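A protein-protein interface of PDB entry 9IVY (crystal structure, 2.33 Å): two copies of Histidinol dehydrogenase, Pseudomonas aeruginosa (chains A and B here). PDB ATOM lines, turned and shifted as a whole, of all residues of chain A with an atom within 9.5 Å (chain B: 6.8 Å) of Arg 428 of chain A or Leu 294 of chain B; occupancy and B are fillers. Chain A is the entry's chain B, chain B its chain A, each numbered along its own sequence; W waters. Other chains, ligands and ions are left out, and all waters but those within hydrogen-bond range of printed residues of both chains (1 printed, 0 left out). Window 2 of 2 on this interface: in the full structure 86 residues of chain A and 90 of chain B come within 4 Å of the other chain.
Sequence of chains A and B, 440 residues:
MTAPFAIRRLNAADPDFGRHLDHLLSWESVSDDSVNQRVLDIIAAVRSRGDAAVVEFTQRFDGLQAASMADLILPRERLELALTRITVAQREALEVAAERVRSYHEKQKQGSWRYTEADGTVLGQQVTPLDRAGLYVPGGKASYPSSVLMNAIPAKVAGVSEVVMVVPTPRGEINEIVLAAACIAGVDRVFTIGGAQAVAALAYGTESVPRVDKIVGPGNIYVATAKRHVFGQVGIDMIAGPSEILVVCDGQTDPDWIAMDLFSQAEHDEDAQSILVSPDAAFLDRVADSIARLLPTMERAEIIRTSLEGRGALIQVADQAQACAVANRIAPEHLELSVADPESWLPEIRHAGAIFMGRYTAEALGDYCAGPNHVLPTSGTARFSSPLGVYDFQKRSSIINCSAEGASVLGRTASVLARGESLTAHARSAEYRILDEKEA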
ATOM      1  N   GLY A 411      30.046  -9.510  26.895  1.00  0.00           N
ATOM      2  CA  GLY A 411      29.743 -10.824  27.433  1.00  0.00           C
ATOM      3  C   GLY A 411      29.008 -10.787  28.758  1.00  0.00           C
ATOM      4  O   GLY A 411      28.201 -11.677  29.045  1.00  0.00           O
ATOM      5  N   ALA A 414      25.484 -10.184  27.672  1.00  0.00           N
ATOM      6  CA  ALA A 414      24.996 -11.385  27.000  1.00  0.00           C
ATOM      7  C   ALA A 414      24.755 -12.514  27.995  1.00  0.00           C
ATOM      8  O   ALA A 414      23.736 -13.208  27.918  1.00  0.00           O
ATOM      9  CB  ALA A 414      25.988 -11.821  25.923  1.00  0.00           C
ATOM     10  N   SER A 415      25.675 -12.697  28.944  1.00  0.00           N
ATOM     11  CA  SER A 415      25.546 -13.764  29.932  1.00  0.00           C
ATOM     12  C   SER A 415      24.277 -13.611  30.762  1.00  0.00           C
ATOM     13  O   SER A 415      23.577 -14.596  31.024  1.00  0.00           O
ATOM     14  CB  SER A 415      26.778 -13.785  30.839  1.00  0.00           C
ATOM     15  OG  SER A 415      26.619 -14.693  31.917  1.00  0.00           O
ATOM     16  N   VAL A 416      23.962 -12.384  31.183  1.00  0.00           N
ATOM     17  CA  VAL A 416      22.772 -12.168  32.002  1.00  0.00           C
ATOM     18  C   VAL A 416      21.521 -12.605  31.249  1.00  0.00           C
ATOM     19  O   VAL A 416      20.680 -13.340  31.779  1.00  0.00           O
ATOM     20  CB  VAL A 416      22.679 -10.696  32.442  1.00  0.00           C
ATOM     21  CG1 VAL A 416      21.317 -10.416  33.061  1.00  0.00           C
ATOM     22  CG2 VAL A 416      23.794 -10.367  33.426  1.00  0.00           C
ATOM     23  N   ALA A 418      21.275 -14.536  28.440  1.00  0.00           N
ATOM     24  CA  ALA A 418      21.300 -15.950  28.065  1.00  0.00           C
ATOM     25  C   ALA A 418      21.010 -16.855  29.259  1.00  0.00           C
ATOM     26  O   ALA A 418      20.246 -17.820  29.137  1.00  0.00           O
ATOM     27  CB  ALA A 418      22.647 -16.310  27.438  1.00  0.00           C
ATOM     28  N   ARG A 419      21.609 -16.569  30.420  1.00  0.00           N
ATOM     29  CA  ARG A 419      21.318 -17.373  31.605  1.00  0.00           C
ATOM     30  C   ARG A 419      19.845 -17.291  31.979  1.00  0.00           C
ATOM     31  O   ARG A 419      19.220 -18.310  32.291  1.00  0.00           O
ATOM     32  CB  ARG A 419      22.189 -16.936  32.782  1.00  0.00           C
ATOM     33  CG  ARG A 419      23.663 -17.220  32.590  1.00  0.00           C
ATOM     34  CD  ARG A 419      24.039 -18.595  33.071  1.00  0.00           C
ATOM     35  NE  ARG A 419      25.482 -18.784  33.023  1.00  0.00           N
ATOM     36  CZ  ARG A 419      26.096 -19.914  33.345  1.00  0.00           C
ATOM     37  NH1 ARG A 419      25.419 -20.962  33.787  1.00  0.00           N
ATOM     38  NH2 ARG A 419      27.419 -19.995  33.215  1.00  0.00           N
ATOM     39  N   SER A 422      17.976 -19.857  30.068  1.00  0.00           N
ATOM     40  CA  SER A 422      18.450 -21.241  30.116  1.00  0.00           C
ATOM     41  C   SER A 422      19.185 -21.640  28.835  1.00  0.00           C
ATOM     42  O   SER A 422      19.224 -22.817  28.472  1.00  0.00           O
ATOM     43  CB  SER A 422      17.297 -22.207  30.404  1.00  0.00           C
ATOM     44  OG  SER A 422      16.818 -22.033  31.728  1.00  0.00           O
ATOM     45  N   LEU A 423      19.775 -20.665  28.147  1.00  0.00           N
ATOM     46  CA  LEU A 423      20.633 -20.924  26.991  1.00  0.00           C
ATOM     47  C   LEU A 423      22.096 -20.899  27.438  1.00  0.00           C
ATOM     48  O   LEU A 423      22.869 -19.992  27.127  1.00  0.00           O
ATOM     49  CB  LEU A 423      20.356 -19.902  25.893  1.00  0.00           C
ATOM     50  CG  LEU A 423      19.005 -20.064  25.196  1.00  0.00           C
ATOM     51  CD1 LEU A 423      18.766 -18.940  24.201  1.00  0.00           C
ATOM     52  CD2 LEU A 423      18.949 -21.401  24.492  1.00  0.00           C
ATOM     53  N   THR A 424      22.468 -21.937  28.188  1.00  0.00           N
ATOM     54  CA  THR A 424      23.741 -21.916  28.900  1.00  0.00           C
ATOM     55  C   THR A 424      24.953 -22.026  27.977  1.00  0.00           C
ATOM     56  O   THR A 424      26.041 -21.587  28.362  1.00  0.00           O
ATOM     57  CB  THR A 424      23.774 -23.035  29.941  1.00  0.00           C
ATOM     58  OG1 THR A 424      23.459 -24.283  29.311  1.00  0.00           O
ATOM     59  CG2 THR A 424      22.761 -22.753  31.048  1.00  0.00           C
ATOM     60  N   ALA A 425      24.801 -22.595  26.776  1.00  0.00           N
ATOM     61  CA  ALA A 425      25.924 -22.600  25.840  1.00  0.00           C
ATOM     62  C   ALA A 425      26.208 -21.193  25.322  1.00  0.00           C
ATOM     63  O   ALA A 425      27.372 -20.785  25.227  1.00  0.00           O
ATOM     64  CB  ALA A 425      25.657 -23.561  24.681  1.00  0.00           C
ATOM     65  N   HIS A 426      25.157 -20.440  24.979  1.00  0.00           N
ATOM     66  CA  HIS A 426      25.316 -19.019  24.687  1.00  0.00           C
ATOM     67  C   HIS A 426      26.085 -18.313  25.790  1.00  0.00           C
ATOM     68  O   HIS A 426      27.050 -17.582  25.527  1.00  0.00           O
ATOM     69  CB  HIS A 426      23.952 -18.360  24.530  1.00  0.00           C
ATOM     70  CG  HIS A 426      23.360 -18.510  23.173  1.00  0.00           C
ATOM     71  ND1 HIS A 426      22.628 -19.616  22.803  1.00  0.00           N
ATOM     72  CD2 HIS A 426      23.387 -17.693  22.095  1.00  0.00           C
ATOM     73  CE1 HIS A 426      22.227 -19.473  21.554  1.00  0.00           C
ATOM     74  NE2 HIS A 426      22.676 -18.316  21.101  1.00  0.00           N
ATOM     75  N   ALA A 427      25.656 -18.516  27.037  1.00  0.00           N
ATOM     76  CA  ALA A 427      26.236 -17.787  28.158  1.00  0.00           C
ATOM     77  C   ALA A 427      27.704 -18.134  28.334  1.00  0.00           C
ATOM     78  O   ALA A 427      28.549 -17.247  28.511  1.00  0.00           O
ATOM     79  CB  ALA A 427      25.454 -18.087  29.437  1.00  0.00           C
ATOM     80  N   ARG A 428      28.030 -19.427  28.276  1.00  0.00           N
ATOM     81  CA  ARG A 428      29.397 -19.839  28.573  1.00  0.00           C
ATOM     82  C   ARG A 428      30.362 -19.451  27.459  1.00  0.00           C
ATOM     83  O   ARG A 428      31.516 -19.110  27.742  1.00  0.00           O
ATOM     84  CB  ARG A 428      29.441 -21.341  28.857  1.00  0.00           C
ATOM     85  CG  ARG A 428      28.874 -21.691  30.234  1.00  0.00           C
ATOM     86  CD  ARG A 428      28.547 -23.163  30.364  1.00  0.00           C
ATOM     87  NE  ARG A 428      29.757 -23.970  30.447  1.00  0.00           N
ATOM     88  CZ  ARG A 428      29.772 -25.270  30.698  1.00  0.00           C
ATOM     89  NH1 ARG A 428      28.652 -25.951  30.888  1.00  0.00           N
ATOM     90  NH2 ARG A 428      30.939 -25.906  30.754  1.00  0.00           N
ATOM     91  N   SER A 429      29.919 -19.461  26.196  1.00  0.00           N
ATOM     92  CA  SER A 429      30.819 -19.016  25.134  1.00  0.00           C
ATOM     93  C   SER A 429      31.147 -17.534  25.273  1.00  0.00           C
ATOM     94  O   SER A 429      32.267 -17.120  24.959  1.00  0.00           O
ATOM     95  CB  SER A 429      30.230 -19.309  23.749  1.00  0.00           C
ATOM     96  OG  SER A 429      29.136 -18.463  23.450  1.00  0.00           O
ATOM     97  N   ALA A 430      30.199 -16.732  25.767  1.00  0.00           N
ATOM     98  CA  ALA A 430      30.482 -15.324  26.033  1.00  0.00           C
ATOM     99  C   ALA A 430      31.344 -15.154  27.281  1.00  0.00           C
ATOM    100  O   ALA A 430      32.255 -14.317  27.305  1.00  0.00           O
ATOM    101  CB  ALA A 430      29.177 -14.542  26.175  1.00  0.00           C
ATOM    102  N   GLU A 431      31.069 -15.940  28.326  1.00  0.00           N
ATOM    103  CA  GLU A 431      31.814 -15.811  29.576  1.00  0.00           C
ATOM    104  C   GLU A 431      33.273 -16.220  29.419  1.00  0.00           C
ATOM    105  O   GLU A 431      34.136 -15.720  30.152  1.00  0.00           O
ATOM    106  CB  GLU A 431      31.148 -16.644  30.672  1.00  0.00           C
ATOM    107  CG  GLU A 431      29.802 -16.103  31.117  1.00  0.00           C
ATOM    108  CD  GLU A 431      28.913 -17.177  31.704  1.00  0.00           C
ATOM    109  OE1 GLU A 431      29.388 -18.322  31.844  1.00  0.00           O
ATOM    110  OE2 GLU A 431      27.741 -16.876  32.026  1.00  0.00           O
ATOM    111  N   TYR A 432      33.568 -17.125  28.479  1.00  0.00           N
ATOM    112  CA  TYR A 432      34.952 -17.524  28.234  1.00  0.00           C
ATOM    113  C   TYR A 432      35.838 -16.327  27.931  1.00  0.00           C
ATOM    114  O   TYR A 432      37.033 -16.340  28.252  1.00  0.00           O
ATOM    115  CB  TYR A 432      35.024 -18.506  27.066  1.00  0.00           C
ATOM    116  CG  TYR A 432      34.851 -19.964  27.426  1.00  0.00           C
ATOM    117  CD1 TYR A 432      35.620 -20.560  28.423  1.00  0.00           C
ATOM    118  CD2 TYR A 432      33.937 -20.756  26.742  1.00  0.00           C
ATOM    119  CE1 TYR A 432      35.463 -21.904  28.736  1.00  0.00           C
ATOM    120  CE2 TYR A 432      33.777 -22.093  27.047  1.00  0.00           C
ATOM    121  CZ  TYR A 432      34.536 -22.664  28.039  1.00  0.00           C
ATOM    122  OH  TYR A 432      34.360 -24.002  28.330  1.00  0.00           O
ATOM    123  N   ARG A 433      35.276 -15.287  27.317  1.00  0.00           N
ATOM    124  CA  ARG A 433      36.037 -14.121  26.895  1.00  0.00           C
ATOM    125  C   ARG A 433      36.000 -12.978  27.901  1.00  0.00           C
ATOM    126  O   ARG A 433      36.691 -11.976  27.695  1.00  0.00           O
ATOM    127  CB  ARG A 433      35.533 -13.635  25.530  1.00  0.00           C
ATOM    128  CG  ARG A 433      36.068 -14.456  24.358  1.00  0.00           C
ATOM    129  CD  ARG A 433      35.104 -15.562  23.941  1.00  0.00           C
ATOM    130  NE  ARG A 433      35.501 -16.166  22.675  1.00  0.00           N
ATOM    131  CZ  ARG A 433      34.878 -17.183  22.096  1.00  0.00           C
ATOM    132  NH1 ARG A 433      33.791 -17.722  22.623  1.00  0.00           N
ATOM    133  NH2 ARG A 433      35.359 -17.674  20.957  1.00  0.00           N
ATOM    134  N   ILE A 434      35.220 -13.094  28.977  1.00  0.00           N
ATOM    135  CA  ILE A 434      35.251 -12.077  30.022  1.00  0.00           C
ATOM    136  C   ILE A 434      36.614 -12.100  30.697  1.00  0.00           C
ATOM    137  O   ILE A 434      37.136 -13.168  31.045  1.00  0.00           O
ATOM    138  CB  ILE A 434      34.124 -12.303  31.038  1.00  0.00           C
ATOM    139  CG1 ILE A 434      32.756 -12.162  30.365  1.00  0.00           C
ATOM    140  CG2 ILE A 434      34.263 -11.329  32.196  1.00  0.00           C
ATOM    141  CD1 ILE A 434      31.601 -12.164  31.344  1.00  0.00           C
ATOM    142  N   PRO B 255      40.310 -24.745  22.504  1.00  0.00           N
ATOM    143  CA  PRO B 255      39.345 -25.696  21.936  1.00  0.00           C
ATOM    144  C   PRO B 255      38.030 -25.735  22.692  1.00  0.00           C
ATOM    145  O   PRO B 255      36.998 -26.048  22.086  1.00  0.00           O
ATOM    146  CB  PRO B 255      40.087 -27.037  22.013  1.00  0.00           C
ATOM    147  CG  PRO B 255      41.031 -26.864  23.182  1.00  0.00           C
ATOM    148  CD  PRO B 255      41.456 -25.416  23.145  1.00  0.00           C
ATOM    149  N   ASP B 256      38.030 -25.423  23.994  1.00  0.00           N
ATOM    150  CA  ASP B 256      36.767 -25.362  24.726  1.00  0.00           C
ATOM    151  C   ASP B 256      35.901 -24.206  24.244  1.00  0.00           C
ATOM    152  O   ASP B 256      34.671 -24.330  24.215  1.00  0.00           O
ATOM    153  CB  ASP B 256      37.018 -25.240  26.228  1.00  0.00           C
ATOM    154  CG  ASP B 256      37.785 -26.416  26.791  1.00  0.00           C
ATOM    155  OD1 ASP B 256      37.530 -27.557  26.355  1.00  0.00           O
ATOM    156  OD2 ASP B 256      38.643 -26.199  27.672  1.00  0.00           O
ATOM    157  N   TRP B 257      36.524 -23.084  23.861  1.00  0.00           N
ATOM    158  CA  TRP B 257      35.772 -21.949  23.331  1.00  0.00           C
ATOM    159  C   TRP B 257      35.076 -22.318  22.027  1.00  0.00           C
ATOM    160  O   TRP B 257      33.902 -21.989  21.820  1.00  0.00           O
ATOM    161  CB  TRP B 257      36.698 -20.756  23.094  1.00  0.00           C
ATOM    162  CG  TRP B 257      37.328 -20.165  24.299  1.00  0.00           C
ATOM    163  CD1 TRP B 257      37.380 -20.699  25.554  1.00  0.00           C
ATOM    164  CD2 TRP B 257      38.015 -18.908  24.367  1.00  0.00           C
ATOM    165  NE1 TRP B 257      38.054 -19.849  26.400  1.00  0.00           N
ATOM    166  CE2 TRP B 257      38.454 -18.742  25.695  1.00  0.00           C
ATOM    167  CE3 TRP B 257      38.297 -17.902  23.431  1.00  0.00           C
ATOM    168  CZ2 TRP B 257      39.161 -17.614  26.112  1.00  0.00           C
ATOM    169  CZ3 TRP B 257      39.004 -16.784  23.846  1.00  0.00           C
ATOM    170  CH2 TRP B 257      39.426 -16.648  25.175  1.00  0.00           C
ATOM    171  N   ALA B 259      34.301 -25.340  20.918  1.00  0.00           N
ATOM    172  CA  ALA B 259      33.234 -26.281  21.243  1.00  0.00           C
ATOM    173  C   ALA B 259      31.999 -25.552  21.759  1.00  0.00           C
ATOM    174  O   ALA B 259      30.876 -25.836  21.332  1.00  0.00           O
ATOM    175  CB  ALA B 259      33.727 -27.300  22.275  1.00  0.00           C
ATOM    176  N   MET B 260      32.189 -24.606  22.681  1.00  0.00           N
ATOM    177  CA  MET B 260      31.055 -23.859  23.220  1.00  0.00           C
ATOM    178  C   MET B 260      30.396 -23.006  22.142  1.00  0.00           C
ATOM    179  O   MET B 260      29.165 -22.903  22.093  1.00  0.00           O
ATOM    180  CB  MET B 260      31.509 -22.983  24.386  1.00  0.00           C
ATOM    181  CG  MET B 260      30.476 -22.749  25.476  1.00  0.00           C
ATOM    182  SD  MET B 260      29.427 -24.153  25.888  1.00  0.00           S
ATOM    183  CE  MET B 260      30.580 -25.153  26.823  1.00  0.00           C
ATOM    184  N   ASP B 261      31.203 -22.391  21.268  1.00  0.00           N
ATOM    185  CA  ASP B 261      30.648 -21.622  20.156  1.00  0.00           C
ATOM    186  C   ASP B 261      29.787 -22.497  19.256  1.00  0.00           C
ATOM    187  O   ASP B 261      28.740 -22.056  18.766  1.00  0.00           O
ATOM    188  CB  ASP B 261      31.769 -20.980  19.339  1.00  0.00           C
ATOM    189  CG  ASP B 261      32.554 -19.961  20.124  1.00  0.00           C
ATOM    190  OD1 ASP B 261      32.033 -19.451  21.136  1.00  0.00           O
ATOM    191  OD2 ASP B 261      33.700 -19.664  19.724  1.00  0.00           O
ATOM    192  N   PHE B 263      28.309 -25.300  20.343  1.00  0.00           N
ATOM    193  CA  PHE B 263      27.178 -25.666  21.192  1.00  0.00           C
ATOM    194  C   PHE B 263      26.122 -24.571  21.230  1.00  0.00           C
ATOM    195  O   PHE B 263      24.927 -24.870  21.318  1.00  0.00           O
ATOM    196  CB  PHE B 263      27.641 -25.948  22.626  1.00  0.00           C
ATOM    197  CG  PHE B 263      28.276 -27.296  22.824  1.00  0.00           C
ATOM    198  CD1 PHE B 263      28.665 -28.073  21.747  1.00  0.00           C
ATOM    199  CD2 PHE B 263      28.492 -27.777  24.103  1.00  0.00           C
ATOM    200  CE1 PHE B 263      29.258 -29.312  21.939  1.00  0.00           C
ATOM    201  CE2 PHE B 263      29.082 -29.009  24.305  1.00  0.00           C
ATOM    202  CZ  PHE B 263      29.464 -29.782  23.220  1.00  0.00           C
ATOM    203  N   ASP B 289      37.589 -33.726  21.441  1.00  0.00           N
ATOM    204  CA  ASP B 289      37.615 -34.115  22.851  1.00  0.00           C
ATOM    205  C   ASP B 289      36.836 -33.130  23.716  1.00  0.00           C
ATOM    206  O   ASP B 289      36.107 -33.542  24.628  1.00  0.00           O
ATOM    207  CB  ASP B 289      39.053 -34.226  23.363  1.00  0.00           C
ATOM    208  CG  ASP B 289      39.927 -35.107  22.491  1.00  0.00           C
ATOM    209  OD1 ASP B 289      39.415 -36.093  21.912  1.00  0.00           O
ATOM    210  OD2 ASP B 289      41.139 -34.820  22.399  1.00  0.00           O
ATOM    211  N   SER B 290      36.985 -31.827  23.456  1.00  0.00           N
ATOM    212  CA  SER B 290      36.233 -30.835  24.220  1.00  0.00           C
ATOM    213  C   SER B 290      34.732 -31.045  24.073  1.00  0.00           C
ATOM    214  O   SER B 290      33.984 -30.925  25.052  1.00  0.00           O
ATOM    215  CB  SER B 290      36.615 -29.423  23.780  1.00  0.00           C
ATOM    216  OG  SER B 290      37.981 -29.164  24.028  1.00  0.00           O
ATOM    217  N   ILE B 291      34.271 -31.359  22.859  1.00  0.00           N
ATOM    218  CA  ILE B 291      32.846 -31.616  22.649  1.00  0.00           C
ATOM    219  C   ILE B 291      32.385 -32.780  23.521  1.00  0.00           C
ATOM    220  O   ILE B 291      31.378 -32.686  24.234  1.00  0.00           O
ATOM    221  CB  ILE B 291      32.561 -31.879  21.158  1.00  0.00           C
ATOM    222  CG1 ILE B 291      32.654 -30.583  20.351  1.00  0.00           C
ATOM    223  CG2 ILE B 291      31.188 -32.488  20.972  1.00  0.00           C
ATOM    224  CD1 ILE B 291      32.947 -30.802  18.897  1.00  0.00           C
ATOM    225  N   ALA B 292      33.128 -33.893  23.482  1.00  0.00           N
ATOM    226  CA  ALA B 292      32.744 -35.080  24.243  1.00  0.00           C
ATOM    227  C   ALA B 292      32.719 -34.805  25.740  1.00  0.00           C
ATOM    228  O   ALA B 292      31.821 -35.275  26.449  1.00  0.00           O
ATOM    229  CB  ALA B 292      33.701 -36.231  23.933  1.00  0.00           C
ATOM    230  N   ARG B 293      33.699 -34.048  26.244  1.00  0.00           N
ATOM    231  CA  ARG B 293      33.765 -33.779  27.677  1.00  0.00           C
ATOM    232  C   ARG B 293      32.715 -32.762  28.110  1.00  0.00           C
ATOM    233  O   ARG B 293      32.129 -32.897  29.190  1.00  0.00           O
ATOM    234  CB  ARG B 293      35.165 -33.292  28.065  1.00  0.00           C
ATOM    235  CG  ARG B 293      35.264 -32.825  29.525  1.00  0.00           C
ATOM    236  CD  ARG B 293      36.630 -32.253  29.911  1.00  0.00           C
ATOM    237  NE  ARG B 293      37.501 -31.996  28.769  1.00  0.00           N
ATOM    238  CZ  ARG B 293      37.802 -30.786  28.318  1.00  0.00           C
ATOM    239  NH1 ARG B 293      37.275 -29.697  28.860  1.00  0.00           N
ATOM    240  NH2 ARG B 293      38.653 -30.665  27.301  1.00  0.00           N
ATOM    241  N   LEU B 294      32.459 -31.744  27.288  1.00  0.00           N
ATOM    242  CA  LEU B 294      31.599 -30.642  27.700  1.00  0.00           C
ATOM    243  C   LEU B 294      30.118 -30.910  27.475  1.00  0.00           C
ATOM    244  O   LEU B 294      29.289 -30.325  28.178  1.00  0.00           O
ATOM    245  CB  LEU B 294      31.999 -29.355  26.969  1.00  0.00           C
ATOM    246  CG  LEU B 294      33.312 -28.714  27.428  1.00  0.00           C
ATOM    247  CD1 LEU B 294      33.818 -27.697  26.409  1.00  0.00           C
ATOM    248  CD2 LEU B 294      33.154 -28.076  28.803  1.00  0.00           C
ATOM    249  N   LEU B 295      29.767 -31.772  26.518  1.00  0.00           N
ATOM    250  CA  LEU B 295      28.356 -32.002  26.204  1.00  0.00           C
ATOM    251  C   LEU B 295      27.536 -32.460  27.405  1.00  0.00           C
ATOM    252  O   LEU B 295      26.455 -31.890  27.631  1.00  0.00           O
ATOM    253  CB  LEU B 295      28.238 -33.000  25.047  1.00  0.00           C
ATOM    254  CG  LEU B 295      26.809 -33.365  24.631  1.00  0.00           C
ATOM    255  CD1 LEU B 295      26.093 -32.155  24.055  1.00  0.00           C
ATOM    256  CD2 LEU B 295      26.794 -34.516  23.635  1.00  0.00           C
ATOM    257  N   PRO B 296      27.959 -33.455  28.202  1.00  0.00           N
ATOM    258  CA  PRO B 296      27.127 -33.866  29.346  1.00  0.00           C
ATOM    259  C   PRO B 296      26.973 -32.795  30.414  1.00  0.00           C
ATOM    260  O   PRO B 296      26.079 -32.920  31.260  1.00  0.00           O
ATOM    261  CB  PRO B 296      27.867 -35.092  29.899  1.00  0.00           C
ATOM    262  CG  PRO B 296      28.717 -35.563  28.771  1.00  0.00           C
ATOM    263  CD  PRO B 296      29.147 -34.317  28.080  1.00  0.00           C
ATOM    264  N   THR B 297      27.806 -31.755  30.411  1.00  0.00           N
ATOM    265  CA  THR B 297      27.639 -30.656  31.355  1.00  0.00           C
ATOM    266  C   THR B 297      26.579 -29.647  30.926  1.00  0.00           C
ATOM    267  O   THR B 297      26.274 -28.735  31.701  1.00  0.00           O
ATOM    268  CB  THR B 297      28.960 -29.911  31.556  1.00  0.00           C
ATOM    269  OG1 THR B 297      29.350 -29.286  30.326  1.00  0.00           O
ATOM    270  CG2 THR B 297      30.058 -30.873  31.992  1.00  0.00           C
ATOM    271  N   MET B 298      26.010 -29.776  29.731  1.00  0.00           N
ATOM    272  CA  MET B 298      25.095 -28.765  29.213  1.00  0.00           C
ATOM    273  C   MET B 298      23.645 -29.131  29.493  1.00  0.00           C
ATOM    274  O   MET B 298      23.231 -30.277  29.291  1.00  0.00           O
ATOM    275  CB  MET B 298      25.320 -28.557  27.718  1.00  0.00           C
ATOM    276  CG  MET B 298      26.781 -28.631  27.356  1.00  0.00           C
ATOM    277  SD  MET B 298      27.673 -27.152  27.904  1.00  0.00           S
ATOM    278  CE  MET B 298      26.463 -25.860  27.618  1.00  0.00           C
ATOM    279  N   GLU B 299      22.882 -28.143  29.963  1.00  0.00           N
ATOM    280  CA  GLU B 299      21.480 -28.370  30.288  1.00  0.00           C
ATOM    281  C   GLU B 299      20.690 -28.786  29.055  1.00  0.00           C
ATOM    282  O   GLU B 299      19.859 -29.699  29.121  1.00  0.00           O
ATOM    283  CB  GLU B 299      20.889 -27.111  30.924  1.00  0.00           C
ATOM    284  CG  GLU B 299      21.413 -26.837  32.337  1.00  0.00           C
ATOM    285  CD  GLU B 299      22.727 -26.049  32.372  1.00  0.00           C
ATOM    286  OE1 GLU B 299      23.563 -26.190  31.450  1.00  0.00           O
ATOM    287  OE2 GLU B 299      22.932 -25.298  33.349  1.00  0.00           O
ATOM    288  N   ALA B 301      21.850 -30.419  26.546  1.00  0.00           N
ATOM    289  CA  ALA B 301      22.702 -31.406  25.880  1.00  0.00           C
ATOM    290  C   ALA B 301      21.929 -32.274  24.899  1.00  0.00           C
ATOM    291  O   ALA B 301      22.485 -32.691  23.876  1.00  0.00           O
ATOM    292  CB  ALA B 301      23.386 -32.299  26.916  1.00  0.00           C
HETATM  293  O   HOH W   1      36.274 -25.289  29.807  1.00  0.00           O
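The side-chain carboxylate of Glu 299 of chain B is in hydrogen-bond range of the side-chain hydroxyl of Thr 424 of chain A, 2.9 Å away. OD2 of Asp 261 of chain B lies within salt-bridge range of NH2 of Arg 433 of chain A. OG1 of Thr 297 of chain B is in hydrogen-bond range of NH1 of Arg 428 of chain A, 3.5 Å away. The side-chain sulfur (SD) of Met 298 of chain B sits at hydrogen-bond distance from the guanidinium group (NH1) of Arg 428 of chain A, at 3.4 Å.
The backbone carbonyl oxygen of His 426 of chain A lies within hydrogen-bond range of the side-chain hydroxyl of Ser 429 of chain A (3.1 Å). The guanidinium group (NH1) of Arg 433 of chain A lies within hydrogen-bond range of the backbone carbonyl oxygen (O) of Ser 429 of chain A (2.9 Å). OD1 of Asp 256 of chain B sits at hydrogen-bond distance from OG of Ser 290 of chain B (2.9 Å). The backbone carbonyl oxygen (O) of Ala 425 of chain A sits at hydrogen-bond distance from the side-chain hydroxyl (OG) of Ser 429 of chain A, at 3.4 Å. The side-chain sulfur (SD) of Met 298 of chain B sits at hydrogen-bond distance from the side-chain hydroxyl (OG1) of Thr 297 of chain B, at 3.6 Å.
Met 298 of chain B touches Thr 424 of chain A (CE to OG1, 3.8 Å). Ala 425 of chain A touches Met 260 of chain B. Ala 425 of chain A touches Phe 263 of chain B (CB to C, 3.6 Å). Met 298 of chain B touches Ala 425 of chain A. Arg 428 of chain A touches Leu 294 of chain B. Asp 261 of chain B touches Ser 429 of chain A. Asp 256 of chain B touches Tyr 432 of chain A. Trp 257 of chain B touches Tyr 432 of chain A (CD1 to CG, 3.2 Å). Tyr 432 of chain A touches Met 260 of chain B. Trp 257 of chain B touches Arg 433 of chain A (CE3 to NE, 3.4 Å).
Of the printed residues of chain B, Thr 424 of chain A touches Met 298 (3.8 Å) and Glu 299 (2.9 Å). Of the printed residues of chain B, Arg 428 of chain A touches Met 260 (3.8 Å), Leu 294 (3.7 Å), Thr 297 (3.5 Å) and Met 298 (3.4 Å). Of the printed residues of chain B, Tyr 432 of chain A touches Asp 256 (3.6 Å), Trp 257 (3.2 Å) and Met 260 (3.6 Å). Printed residues of chain B within 4 Å of Arg 433 of chain A: Trp 257 (3.4 Å) and Asp 261 (2.9 Å). Leu 294 of chain B touches just one residue of chain A: Arg 428 (3.7 Å). Pro 296 of chain B touches none of the printed residues of chain A. The nearest residue of chain B that does not touch Arg 428 of chain A is Glu 299 of chain B (5.1 Å). The nearest residue of chain A that does not touch Leu 294 of chain B is Tyr 432 of chain A (4.2 Å). The nearest printed residue of chain B that does not touch Thr 424 of chain A is Met 260 of chain B (4.9 Å).
Printed residues of chain B that touch a printed residue of chain A: Asp 256, Trp 257, Met 260, Asp 261, Phe 263, Leu 294, Thr 297, Met 298 and Glu 299. Hydrophobic or aromatic side chains of chain A that line the printed part of chain B: Ala 425 and Tyr 432. Among the printed residues, Asp or Glu carboxylates within 4 Å of a Lys or Arg side-chain nitrogen of the other chain: Arg 433 of chain A with Asp 261 of chain B (2.9 Å).
No position is printed for both chains. Of the 16 pairs that touch across the chains among the printed residues, none has its exchanged pair printed and touching as well.
Water W1 bridges the side-chain hydroxyl of Tyr 432 of chain A (2.7 Å) and the side-chain carboxylate of Asp 256 of chain B (3.3 Å).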
